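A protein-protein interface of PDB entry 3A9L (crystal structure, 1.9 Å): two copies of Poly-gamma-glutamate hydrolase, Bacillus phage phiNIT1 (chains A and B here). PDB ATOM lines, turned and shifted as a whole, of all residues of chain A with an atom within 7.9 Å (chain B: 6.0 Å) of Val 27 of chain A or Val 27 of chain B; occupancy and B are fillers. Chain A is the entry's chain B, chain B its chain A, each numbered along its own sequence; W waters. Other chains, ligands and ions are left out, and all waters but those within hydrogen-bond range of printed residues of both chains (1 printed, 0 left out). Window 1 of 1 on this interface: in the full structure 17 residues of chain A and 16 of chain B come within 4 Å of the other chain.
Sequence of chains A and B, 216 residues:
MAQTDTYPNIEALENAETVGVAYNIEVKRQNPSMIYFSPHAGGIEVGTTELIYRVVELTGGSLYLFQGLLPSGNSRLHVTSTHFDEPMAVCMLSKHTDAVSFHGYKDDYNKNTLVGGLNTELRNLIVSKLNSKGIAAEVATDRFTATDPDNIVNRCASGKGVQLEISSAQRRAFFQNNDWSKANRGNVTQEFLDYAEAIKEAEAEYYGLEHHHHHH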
ATOM      1  N   ASN A  24      -6.459  16.935 -18.845  1.00  0.00           N
ATOM      2  CA  ASN A  24      -6.345  15.468 -18.734  1.00  0.00           C
ATOM      3  C   ASN A  24      -7.062  14.855 -19.936  1.00  0.00           C
ATOM      4  O   ASN A  24      -7.719  15.585 -20.706  1.00  0.00           O
ATOM      5  CB  ASN A  24      -6.776  14.910 -17.337  1.00  0.00           C
ATOM      6  CG  ASN A  24      -8.297  14.859 -17.124  1.00  0.00           C
ATOM      7  OD1 ASN A  24      -9.091  14.956 -18.072  1.00  0.00           O
ATOM      8  ND2 ASN A  24      -8.703  14.671 -15.861  1.00  0.00           N
ATOM      9  N   ILE A  25      -6.892  13.541 -20.113  1.00  0.00           N
ATOM     10  CA  ILE A  25      -7.469  12.795 -21.215  1.00  0.00           C
ATOM     11  C   ILE A  25      -8.051  11.536 -20.565  1.00  0.00           C
ATOM     12  O   ILE A  25      -7.360  10.870 -19.770  1.00  0.00           O
ATOM     13  CB  ILE A  25      -6.418  12.381 -22.291  1.00  0.00           C
ATOM     14  CG1 ILE A  25      -5.526  13.582 -22.686  1.00  0.00           C
ATOM     15  CG2 ILE A  25      -7.153  11.707 -23.482  1.00  0.00           C
ATOM     16  CD1 ILE A  25      -4.546  13.420 -23.868  1.00  0.00           C
ATOM     17  N   GLU A  26      -9.311  11.261 -20.884  1.00  0.00           N
ATOM     18  CA  GLU A  26     -10.035  10.048 -20.458  1.00  0.00           C
ATOM     19  C   GLU A  26     -10.520   9.300 -21.668  1.00  0.00           C
ATOM     20  O   GLU A  26     -11.091   9.883 -22.579  1.00  0.00           O
ATOM     21  CB  GLU A  26     -11.289  10.410 -19.663  1.00  0.00           C
ATOM     22  CG  GLU A  26     -11.065  11.252 -18.465  1.00  0.00           C
ATOM     23  CD  GLU A  26     -12.325  11.452 -17.654  1.00  0.00           C
ATOM     24  OE1 GLU A  26     -13.448  11.135 -18.120  1.00  0.00           O
ATOM     25  OE2 GLU A  26     -12.188  11.929 -16.524  1.00  0.00           O
ATOM     26  N   VAL A  27     -10.353   7.989 -21.638  1.00  0.00           N
ATOM     27  CA  VAL A  27     -10.624   7.144 -22.768  1.00  0.00           C
ATOM     28  C   VAL A  27     -11.284   5.898 -22.228  1.00  0.00           C
ATOM     29  O   VAL A  27     -10.897   5.407 -21.173  1.00  0.00           O
ATOM     30  CB  VAL A  27      -9.289   6.751 -23.491  1.00  0.00           C
ATOM     31  CG1 VAL A  27      -9.588   6.116 -24.812  1.00  0.00           C
ATOM     32  CG2 VAL A  27      -8.397   7.963 -23.732  1.00  0.00           C
ATOM     33  N   LYS A  28     -12.307   5.399 -22.917  1.00  0.00           N
ATOM     34  CA  LYS A  28     -12.868   4.083 -22.605  1.00  0.00           C
ATOM     35  C   LYS A  28     -13.303   3.469 -23.905  1.00  0.00           C
ATOM     36  O   LYS A  28     -14.341   3.850 -24.442  1.00  0.00           O
ATOM     37  CB  LYS A  28     -14.083   4.160 -21.668  1.00  0.00           C
ATOM     38  CG  LYS A  28     -14.522   2.748 -21.129  1.00  0.00           C
ATOM     39  CD  LYS A  28     -15.779   2.809 -20.331  1.00  0.00           C
ATOM     40  CE  LYS A  28     -15.928   1.599 -19.390  1.00  0.00           C
ATOM     41  NZ  LYS A  28     -17.282   1.589 -18.771  1.00  0.00           N
ATOM     42  N   ARG A  29     -12.519   2.515 -24.399  1.00  0.00           N
ATOM     43  CA  ARG A  29     -12.794   1.847 -25.660  1.00  0.00           C
ATOM     44  C   ARG A  29     -13.577   0.563 -25.406  1.00  0.00           C
ATOM     45  O   ARG A  29     -13.038  -0.430 -24.856  1.00  0.00           O
ATOM     46  CB  ARG A  29     -11.507   1.520 -26.408  1.00  0.00           C
ATOM     47  CG  ARG A  29     -11.806   1.176 -27.898  1.00  0.00           C
ATOM     48  CD  ARG A  29     -10.652   0.491 -28.579  1.00  0.00           C
ATOM     49  NE  ARG A  29     -11.101  -0.207 -29.800  1.00  0.00           N
ATOM     50  CZ  ARG A  29     -10.356  -1.032 -30.548  1.00  0.00           C
ATOM     51  NH1 ARG A  29      -9.089  -1.274 -30.252  1.00  0.00           N
ATOM     52  NH2 ARG A  29     -10.881  -1.615 -31.625  1.00  0.00           N
ATOM     53  N   GLN A  30     -14.850   0.590 -25.781  1.00  0.00           N
ATOM     54  CA  GLN A  30     -15.732  -0.522 -25.401  1.00  0.00           C
ATOM     55  C   GLN A  30     -16.830  -0.831 -26.446  1.00  0.00           C
ATOM     56  O   GLN A  30     -17.771  -1.582 -26.168  1.00  0.00           O
ATOM     57  CB  GLN A  30     -16.311  -0.271 -24.012  1.00  0.00           C
ATOM     58  CG  GLN A  30     -17.306   0.916 -23.981  1.00  0.00           C
ATOM     59  CD  GLN A  30     -18.047   1.092 -22.687  1.00  0.00           C
ATOM     60  OE1 GLN A  30     -17.901   0.307 -21.760  1.00  0.00           O
ATOM     61  NE2 GLN A  30     -18.866   2.165 -22.606  1.00  0.00           N
ATOM     62  N   ILE A  35     -18.256   5.890 -31.239  1.00  0.00           N
ATOM     63  CA  ILE A  35     -17.524   6.629 -30.181  1.00  0.00           C
ATOM     64  C   ILE A  35     -18.124   8.024 -30.096  1.00  0.00           C
ATOM     65  O   ILE A  35     -18.407   8.694 -31.132  1.00  0.00           O
ATOM     66  CB  ILE A  35     -15.959   6.708 -30.400  1.00  0.00           C
ATOM     67  CG1 ILE A  35     -15.298   7.516 -29.244  1.00  0.00           C
ATOM     68  CG2 ILE A  35     -15.665   7.275 -31.820  1.00  0.00           C
ATOM     69  CD1 ILE A  35     -13.732   7.549 -29.149  1.00  0.00           C
ATOM     70  N   SER A  62     -18.046   3.826 -27.086  1.00  0.00           N
ATOM     71  CA  SER A  62     -16.732   4.189 -26.502  1.00  0.00           C
ATOM     72  C   SER A  62     -16.716   5.677 -26.117  1.00  0.00           C
ATOM     73  O   SER A  62     -17.522   6.466 -26.645  1.00  0.00           O
ATOM     74  CB  SER A  62     -15.560   3.867 -27.426  1.00  0.00           C
ATOM     75  OG  SER A  62     -15.504   2.482 -27.800  1.00  0.00           O
ATOM     76  N   LEU A  63     -15.840   6.055 -25.174  1.00  0.00           N
ATOM     77  CA  LEU A  63     -15.697   7.475 -24.762  1.00  0.00           C
ATOM     78  C   LEU A  63     -14.277   8.016 -25.051  1.00  0.00           C
ATOM     79  O   LEU A  63     -13.304   7.260 -24.993  1.00  0.00           O
ATOM     80  CB  LEU A  63     -16.055   7.627 -23.289  1.00  0.00           C
ATOM     81  CG  LEU A  63     -15.714   8.835 -22.393  1.00  0.00           C
ATOM     82  CD1 LEU A  63     -16.710   8.917 -21.274  1.00  0.00           C
ATOM     83  CD2 LEU A  63     -14.285   8.643 -21.874  1.00  0.00           C
ATOM     84  N   TYR A  64     -14.171   9.320 -25.370  1.00  0.00           N
ATOM     85  CA  TYR A  64     -12.883  10.024 -25.358  1.00  0.00           C
ATOM     86  C   TYR A  64     -13.138  11.455 -24.905  1.00  0.00           C
ATOM     87  O   TYR A  64     -14.037  12.076 -25.433  1.00  0.00           O
ATOM     88  CB  TYR A  64     -12.162   9.978 -26.736  1.00  0.00           C
ATOM     89  CG  TYR A  64     -10.920  10.870 -26.800  1.00  0.00           C
ATOM     90  CD1 TYR A  64     -11.033  12.231 -27.097  1.00  0.00           C
ATOM     91  CD2 TYR A  64      -9.641  10.354 -26.538  1.00  0.00           C
ATOM     92  CE1 TYR A  64      -9.903  13.061 -27.143  1.00  0.00           C
ATOM     93  CE2 TYR A  64      -8.512  11.165 -26.544  1.00  0.00           C
ATOM     94  CZ  TYR A  64      -8.650  12.529 -26.866  1.00  0.00           C
ATOM     95  OH  TYR A  64      -7.535  13.320 -26.904  1.00  0.00           O
ATOM     96  N   LEU A  65     -12.426  11.947 -23.875  1.00  0.00           N
ATOM     97  CA  LEU A  65     -12.535  13.374 -23.503  1.00  0.00           C
ATOM     98  C   LEU A  65     -11.172  14.030 -23.371  1.00  0.00           C
ATOM     99  O   LEU A  65     -10.299  13.529 -22.680  1.00  0.00           O
ATOM    100  CB  LEU A  65     -13.328  13.575 -22.197  1.00  0.00           C
ATOM    101  CG  LEU A  65     -14.771  13.105 -22.050  1.00  0.00           C
ATOM    102  CD1 LEU A  65     -15.202  13.147 -20.627  1.00  0.00           C
ATOM    103  CD2 LEU A  65     -15.697  13.902 -22.931  1.00  0.00           C
ATOM    104  N   PHE A  66     -10.972  15.111 -24.108  1.00  0.00           N
ATOM    105  CA  PHE A  66      -9.873  16.015 -23.838  1.00  0.00           C
ATOM    106  C   PHE A  66     -10.386  17.167 -22.965  1.00  0.00           C
ATOM    107  O   PHE A  66     -10.983  18.140 -23.465  1.00  0.00           O
ATOM    108  CB  PHE A  66      -9.262  16.564 -25.135  1.00  0.00           C
ATOM    109  CG  PHE A  66      -7.946  17.270 -24.918  1.00  0.00           C
ATOM    110  CD1 PHE A  66      -6.755  16.550 -24.937  1.00  0.00           C
ATOM    111  CD2 PHE A  66      -7.907  18.656 -24.676  1.00  0.00           C
ATOM    112  CE1 PHE A  66      -5.553  17.180 -24.715  1.00  0.00           C
ATOM    113  CE2 PHE A  66      -6.696  19.299 -24.456  1.00  0.00           C
ATOM    114  CZ  PHE A  66      -5.519  18.563 -24.477  1.00  0.00           C
ATOM    115  N   GLU A  86      -4.484  14.873 -31.164  1.00  0.00           N
ATOM    116  CA  GLU A  86      -3.996  14.105 -30.003  1.00  0.00           C
ATOM    117  C   GLU A  86      -3.974  12.624 -30.400  1.00  0.00           C
ATOM    118  O   GLU A  86      -5.016  12.081 -30.839  1.00  0.00           O
ATOM    119  CB  GLU A  86      -4.852  14.348 -28.767  1.00  0.00           C
ATOM    120  CG  GLU A  86      -4.258  13.836 -27.453  1.00  0.00           C
ATOM    121  CD  GLU A  86      -4.419  12.331 -27.308  1.00  0.00           C
ATOM    122  OE1 GLU A  86      -5.545  11.824 -27.445  1.00  0.00           O
ATOM    123  OE2 GLU A  86      -3.396  11.661 -27.110  1.00  0.00           O
ATOM    124  N   MET A  88      -3.969   9.611 -29.115  1.00  0.00           N
ATOM    125  CA  MET A  88      -4.895   8.595 -28.587  1.00  0.00           C
ATOM    126  C   MET A  88      -6.295   8.748 -29.205  1.00  0.00           C
ATOM    127  O   MET A  88      -6.912   7.763 -29.615  1.00  0.00           O
ATOM    128  CB  MET A  88      -4.957   8.585 -27.063  1.00  0.00           C
ATOM    129  CG  MET A  88      -3.709   8.048 -26.434  1.00  0.00           C
ATOM    130  SD  MET A  88      -3.844   7.711 -24.662  1.00  0.00           S
ATOM    131  CE  MET A  88      -4.649   9.174 -23.983  1.00  0.00           C
ATOM    132  N   ALA A  89      -6.772   9.989 -29.279  1.00  0.00           N
ATOM    133  CA  ALA A  89      -8.006  10.302 -29.997  1.00  0.00           C
ATOM    134  C   ALA A  89      -7.969   9.882 -31.445  1.00  0.00           C
ATOM    135  O   ALA A  89      -8.968   9.389 -31.936  1.00  0.00           O
ATOM    136  CB  ALA A  89      -8.354  11.796 -29.925  1.00  0.00           C
ATOM    137  N   CYS A  91      -6.084   7.557 -32.599  1.00  0.00           N
ATOM    138  CA  CYS A  91      -6.089   6.092 -32.517  1.00  0.00           C
ATOM    139  C   CYS A  91      -7.506   5.579 -32.335  1.00  0.00           C
ATOM    140  O   CYS A  91      -7.977   4.778 -33.145  1.00  0.00           O
ATOM    141  CB  CYS A  91      -5.195   5.574 -31.388  1.00  0.00           C
ATOM    142  SG  CYS A  91      -4.628   3.873 -31.633  1.00  0.00           S
ATOM    143  N   MET A  92      -8.170   6.027 -31.263  1.00  0.00           N
ATOM    144  CA  MET A  92      -9.588   5.714 -31.016  1.00  0.00           C
ATOM    145  C   MET A  92     -10.511   5.825 -32.241  1.00  0.00           C
ATOM    146  O   MET A  92     -11.245   4.885 -32.574  1.00  0.00           O
ATOM    147  CB  MET A  92     -10.135   6.577 -29.880  1.00  0.00           C
ATOM    148  CG  MET A  92      -9.605   6.140 -28.523  1.00  0.00           C
ATOM    149  SD  MET A  92     -10.363   4.556 -28.063  1.00  0.00           S
ATOM    150  CE  MET A  92     -11.827   5.234 -27.308  1.00  0.00           C
ATOM    151  N   HIS A  96     -13.208   2.856 -34.915  1.00  0.00           N
ATOM    152  CA  HIS A  96     -14.680   2.955 -34.777  1.00  0.00           C
ATOM    153  C   HIS A  96     -15.325   3.364 -36.079  1.00  0.00           C
ATOM    154  O   HIS A  96     -14.928   4.359 -36.692  1.00  0.00           O
ATOM    155  CB  HIS A  96     -15.093   4.022 -33.738  1.00  0.00           C
ATOM    156  CG  HIS A  96     -14.766   3.659 -32.334  1.00  0.00           C
ATOM    157  ND1 HIS A  96     -13.504   3.823 -31.808  1.00  0.00           N
ATOM    158  CD2 HIS A  96     -15.523   3.121 -31.344  1.00  0.00           C
ATOM    159  CE1 HIS A  96     -13.502   3.417 -30.546  1.00  0.00           C
ATOM    160  NE2 HIS A  96     -14.713   2.995 -30.240  1.00  0.00           N
ATOM    161  N   ILE B  25     -10.669  -1.205 -23.114  1.00  0.00           N
ATOM    162  CA  ILE B  25      -9.506  -0.451 -22.694  1.00  0.00           C
ATOM    163  C   ILE B  25      -9.948   0.849 -21.998  1.00  0.00           C
ATOM    164  O   ILE B  25     -10.854   1.575 -22.479  1.00  0.00           O
ATOM    165  CB  ILE B  25      -8.571  -0.116 -23.887  1.00  0.00           C
ATOM    166  CG1 ILE B  25      -8.384  -1.339 -24.826  1.00  0.00           C
ATOM    167  CG2 ILE B  25      -7.201   0.377 -23.366  1.00  0.00           C
ATOM    168  CD1 ILE B  25      -7.540  -1.061 -26.064  1.00  0.00           C
ATOM    169  N   GLU B  26      -9.278   1.152 -20.889  1.00  0.00           N
ATOM    170  CA  GLU B  26      -9.548   2.337 -20.063  1.00  0.00           C
ATOM    171  C   GLU B  26      -8.261   3.127 -19.866  1.00  0.00           C
ATOM    172  O   GLU B  26      -7.199   2.548 -19.589  1.00  0.00           O
ATOM    173  CB  GLU B  26     -10.100   1.930 -18.686  1.00  0.00           C
ATOM    174  CG  GLU B  26     -11.394   1.148 -18.687  1.00  0.00           C
ATOM    175  CD  GLU B  26     -12.078   1.188 -17.318  1.00  0.00           C
ATOM    176  OE1 GLU B  26     -11.393   1.360 -16.284  1.00  0.00           O
ATOM    177  OE2 GLU B  26     -13.307   1.079 -17.270  1.00  0.00           O
ATOM    178  N   VAL B  27      -8.337   4.461 -19.975  1.00  0.00           N
ATOM    179  CA  VAL B  27      -7.130   5.323 -19.842  1.00  0.00           C
ATOM    180  C   VAL B  27      -7.521   6.605 -19.102  1.00  0.00           C
ATOM    181  O   VAL B  27      -8.529   7.220 -19.406  1.00  0.00           O
ATOM    182  CB  VAL B  27      -6.548   5.733 -21.225  1.00  0.00           C
ATOM    183  CG1 VAL B  27      -5.258   6.551 -21.071  1.00  0.00           C
ATOM    184  CG2 VAL B  27      -6.294   4.546 -22.138  1.00  0.00           C
ATOM    185  N   LYS B  28      -6.720   7.014 -18.130  1.00  0.00           N
ATOM    186  CA  LYS B  28      -6.833   8.355 -17.644  1.00  0.00           C
ATOM    187  C   LYS B  28      -5.430   8.915 -17.481  1.00  0.00           C
ATOM    188  O   LYS B  28      -4.715   8.500 -16.594  1.00  0.00           O
ATOM    189  CB  LYS B  28      -7.653   8.424 -16.321  1.00  0.00           C
ATOM    190  CG  LYS B  28      -7.908   9.926 -15.871  1.00  0.00           C
ATOM    191  CD  LYS B  28      -8.662  10.027 -14.558  1.00  0.00           C
ATOM    192  CE  LYS B  28      -9.143  11.473 -14.296  1.00  0.00           C
ATOM    193  NZ  LYS B  28      -9.949  11.607 -13.039  1.00  0.00           N
ATOM    194  N   ARG B  29      -5.041   9.827 -18.370  1.00  0.00           N
ATOM    195  CA  ARG B  29      -3.759  10.482 -18.311  1.00  0.00           C
ATOM    196  C   ARG B  29      -3.992  11.785 -17.532  1.00  0.00           C
ATOM    197  O   ARG B  29      -4.769  12.650 -17.979  1.00  0.00           O
ATOM    198  CB  ARG B  29      -3.224  10.757 -19.731  1.00  0.00           C
ATOM    199  CG  ARG B  29      -1.765  11.198 -19.691  1.00  0.00           C
ATOM    200  CD  ARG B  29      -1.144  11.579 -21.031  1.00  0.00           C
ATOM    201  NE  ARG B  29       0.132  12.252 -20.793  1.00  0.00           N
ATOM    202  CZ  ARG B  29       0.724  13.123 -21.612  1.00  0.00           C
ATOM    203  NH1 ARG B  29       0.215  13.399 -22.786  1.00  0.00           N
ATOM    204  NH2 ARG B  29       1.874  13.686 -21.259  1.00  0.00           N
ATOM    205  N   LEU B  63      -3.775   6.196 -15.142  1.00  0.00           N
ATOM    206  CA  LEU B  63      -4.301   4.839 -15.144  1.00  0.00           C
ATOM    207  C   LEU B  63      -4.369   4.338 -16.574  1.00  0.00           C
ATOM    208  O   LEU B  63      -4.695   5.093 -17.499  1.00  0.00           O
ATOM    209  CB  LEU B  63      -5.720   4.835 -14.534  1.00  0.00           C
ATOM    210  CG  LEU B  63      -6.681   3.638 -14.606  1.00  0.00           C
ATOM    211  CD1 LEU B  63      -7.689   3.635 -13.437  1.00  0.00           C
ATOM    212  CD2 LEU B  63      -7.411   3.525 -15.955  1.00  0.00           C
ATOM    213  N   TYR B  64      -4.070   3.051 -16.755  1.00  0.00           N
ATOM    214  CA  TYR B  64      -4.359   2.366 -18.016  1.00  0.00           C
ATOM    215  C   TYR B  64      -4.706   0.957 -17.648  1.00  0.00           C
ATOM    216  O   TYR B  64      -3.996   0.385 -16.825  1.00  0.00           O
ATOM    217  CB  TYR B  64      -3.139   2.337 -18.922  1.00  0.00           C
ATOM    218  CG  TYR B  64      -3.327   1.423 -20.116  1.00  0.00           C
ATOM    219  CD1 TYR B  64      -3.045   0.049 -20.021  1.00  0.00           C
ATOM    220  CD2 TYR B  64      -3.780   1.915 -21.320  1.00  0.00           C
ATOM    221  CE1 TYR B  64      -3.208  -0.774 -21.081  1.00  0.00           C
ATOM    222  CE2 TYR B  64      -3.935   1.088 -22.406  1.00  0.00           C
ATOM    223  CZ  TYR B  64      -3.660  -0.246 -22.274  1.00  0.00           C
ATOM    224  OH  TYR B  64      -3.833  -1.087 -23.322  1.00  0.00           O
ATOM    225  N   LEU B  65      -5.763   0.405 -18.256  1.00  0.00           N
ATOM    226  CA  LEU B  65      -6.177  -1.000 -18.031  1.00  0.00           C
ATOM    227  C   LEU B  65      -6.636  -1.673 -19.307  1.00  0.00           C
ATOM    228  O   LEU B  65      -7.596  -1.218 -19.933  1.00  0.00           O
ATOM    229  CB  LEU B  65      -7.368  -1.044 -17.081  1.00  0.00           C
ATOM    230  CG  LEU B  65      -7.309  -0.500 -15.686  1.00  0.00           C
ATOM    231  CD1 LEU B  65      -8.701  -0.568 -15.144  1.00  0.00           C
ATOM    232  CD2 LEU B  65      -6.341  -1.345 -14.826  1.00  0.00           C
ATOM    233  N   MET B  88      -2.172   2.296 -27.455  1.00  0.00           N
ATOM    234  CA  MET B  88      -2.482   3.376 -26.537  1.00  0.00           C
ATOM    235  C   MET B  88      -1.632   3.277 -25.272  1.00  0.00           C
ATOM    236  O   MET B  88      -1.140   4.299 -24.794  1.00  0.00           O
ATOM    237  CB  MET B  88      -3.970   3.461 -26.263  1.00  0.00           C
ATOM    238  CG  MET B  88      -4.746   3.922 -27.455  1.00  0.00           C
ATOM    239  SD  MET B  88      -6.385   4.391 -26.928  1.00  0.00           S
ATOM    240  CE  MET B  88      -6.996   2.778 -26.414  1.00  0.00           C
ATOM    241  N   MET B  92       0.948   5.913 -23.813  1.00  0.00           N
ATOM    242  CA  MET B  92       0.887   6.320 -22.408  1.00  0.00           C
ATOM    243  C   MET B  92       2.219   6.093 -21.691  1.00  0.00           C
ATOM    244  O   MET B  92       2.774   7.005 -21.089  1.00  0.00           O
ATOM    245  CB  MET B  92      -0.245   5.581 -21.680  1.00  0.00           C
ATOM    246  CG  MET B  92      -1.606   6.105 -22.030  1.00  0.00           C
ATOM    247  SD  MET B  92      -1.835   7.741 -21.281  1.00  0.00           S
ATOM    248  CE  MET B  92      -2.055   7.355 -19.566  1.00  0.00           C
HETATM  249  O   HOH W   1     -10.862  14.209 -14.220  1.00  0.00           O
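Water W1 lies within hydrogen-bond range of ND2 of Asn 24 of chain A and NZ of Lys 28 of chain B.
Glu 26 of chain A touches Val 27 of chain B, and with the chains exchanged Val 27 of chain A touches Glu 26 of chain B. Glu 26 of chain A touches Lys 28 of chain B, and with the chains exchanged Lys 28 of chain A touches Glu 26 of chain B. Val 27 of chain B touches its own counterpart, Val 27 of chain A. Met 88 of chain A touches Val 27 of chain B, but with the chains exchanged Val 27 of chain A does not touch Met 88 of chain B (4.2 Å). 10 positions are printed for both chains.
N of Met 88 of chain A is in hydrogen-bond range of OE2 of Glu 86 of chain A (2.9 Å). O of Met 92 of chain A lies within hydrogen-bond range of ND1 of His 96 of chain A (2.6 Å). The backbone carbonyl oxygen (O) of Glu 26 of chain A sits at hydrogen-bond distance from the backbone NH (N) of Leu 65 of chain A, at 2.8 Å. The backbone carbonyl oxygen (O) of Glu 26 of chain B is in hydrogen-bond range of the backbone NH (N) of Leu 65 of chain B, at 2.9 Å. N of Leu 63 of chain A sits at hydrogen-bond distance from O of Lys 28 of chain A (2.8 Å). O of Leu 63 of chain B lies within hydrogen-bond range of N of Lys 28 of chain B (2.9 Å).
Printed residues of chain A within 4 Å of Val 27 of chain B: Ile 25, Glu 26, Val 27 and Met 88. Of the printed residues of chain A, Glu 26 of chain B touches Val 27 and Lys 28. Printed residues of chain A within 4 Å of Met 92 of chain B: Met 88 (3.8 Å). Printed residues of chain B within 4 Å of Glu 26 of chain A: Val 27 (3.4 Å) and Lys 28 (3.8 Å). Of the printed residues of chain A, Ile 25 of chain B touches Lys 28 and Arg 29. Printed residues of chain B within 4 Å of Lys 28 of chain A: Ile 25 and Glu 26. Ser 62 of chain A touches none of the printed residues of chain B. Glu 86 of chain A touches none of the printed residues of chain B. The nearest residue of chain B that does not touch Val 27 of chain A is Ile 25 of chain B (4.05 Å). The nearest residue of chain A that does not touch Val 27 of chain B is Lys 28 of chain A (5.0 Å).
The backbone carbonyl oxygen (O) of Ile 25 of chain B is in hydrogen-bond range of the backbone NH (N) of Arg 29 of chain A, 2.7 Å away. The backbone carbonyl oxygen (O) of Ile 25 of chain A is in hydrogen-bond range of the backbone NH (N) of Arg 29 of chain B (2.9 Å). The backbone NH of Val 27 of chain B lies within hydrogen-bond range of the backbone carbonyl oxygen of Val 27 of chain A (3.0 Å).
Asn 24 of chain A touches Lys 28 of chain B (ND2 to CE, 3.6 Å). Asn 24 of chain A touches Arg 29 of chain B (CB to O, 3.1 Å). Val 27 of chain B touches Ile 25 of chain A. Lys 28 of chain B touches Ile 25 of chain A. Glu 26 of chain A touches Val 27 of chain B. OE2 of Glu 26 of chain A touches CE of Lys 28 of chain B, at 3.8 Å. O of Val 27 of chain A touches CA of Glu 26 of chain B, at 3.5 Å. Ile 25 of chain B touches Lys 28 of chain A (O to CA, 3.2 Å). CE of Met 88 of chain A touches CG1 of Val 27 of chain B, 3.97 Å away. Met 88 of chain B touches Met 92 of chain A.
Of the 10 printed residues of chain B, 7 touch a printed residue of chain A. Hydrophobic or aromatic side chains of chain B within 4 Å of the printed part of chain A: Val 27, Met 88 and Met 92. Along chain B the printed residues that touch a printed residue of chain A span positions 25 to 92. Of the 19 printed residues of chain A, 8 touch a printed residue of chain B. Among the printed residues, no Asp or Glu carboxylate lies within 4 Å of a Lys or Arg side-chain nitrogen of the other chain.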
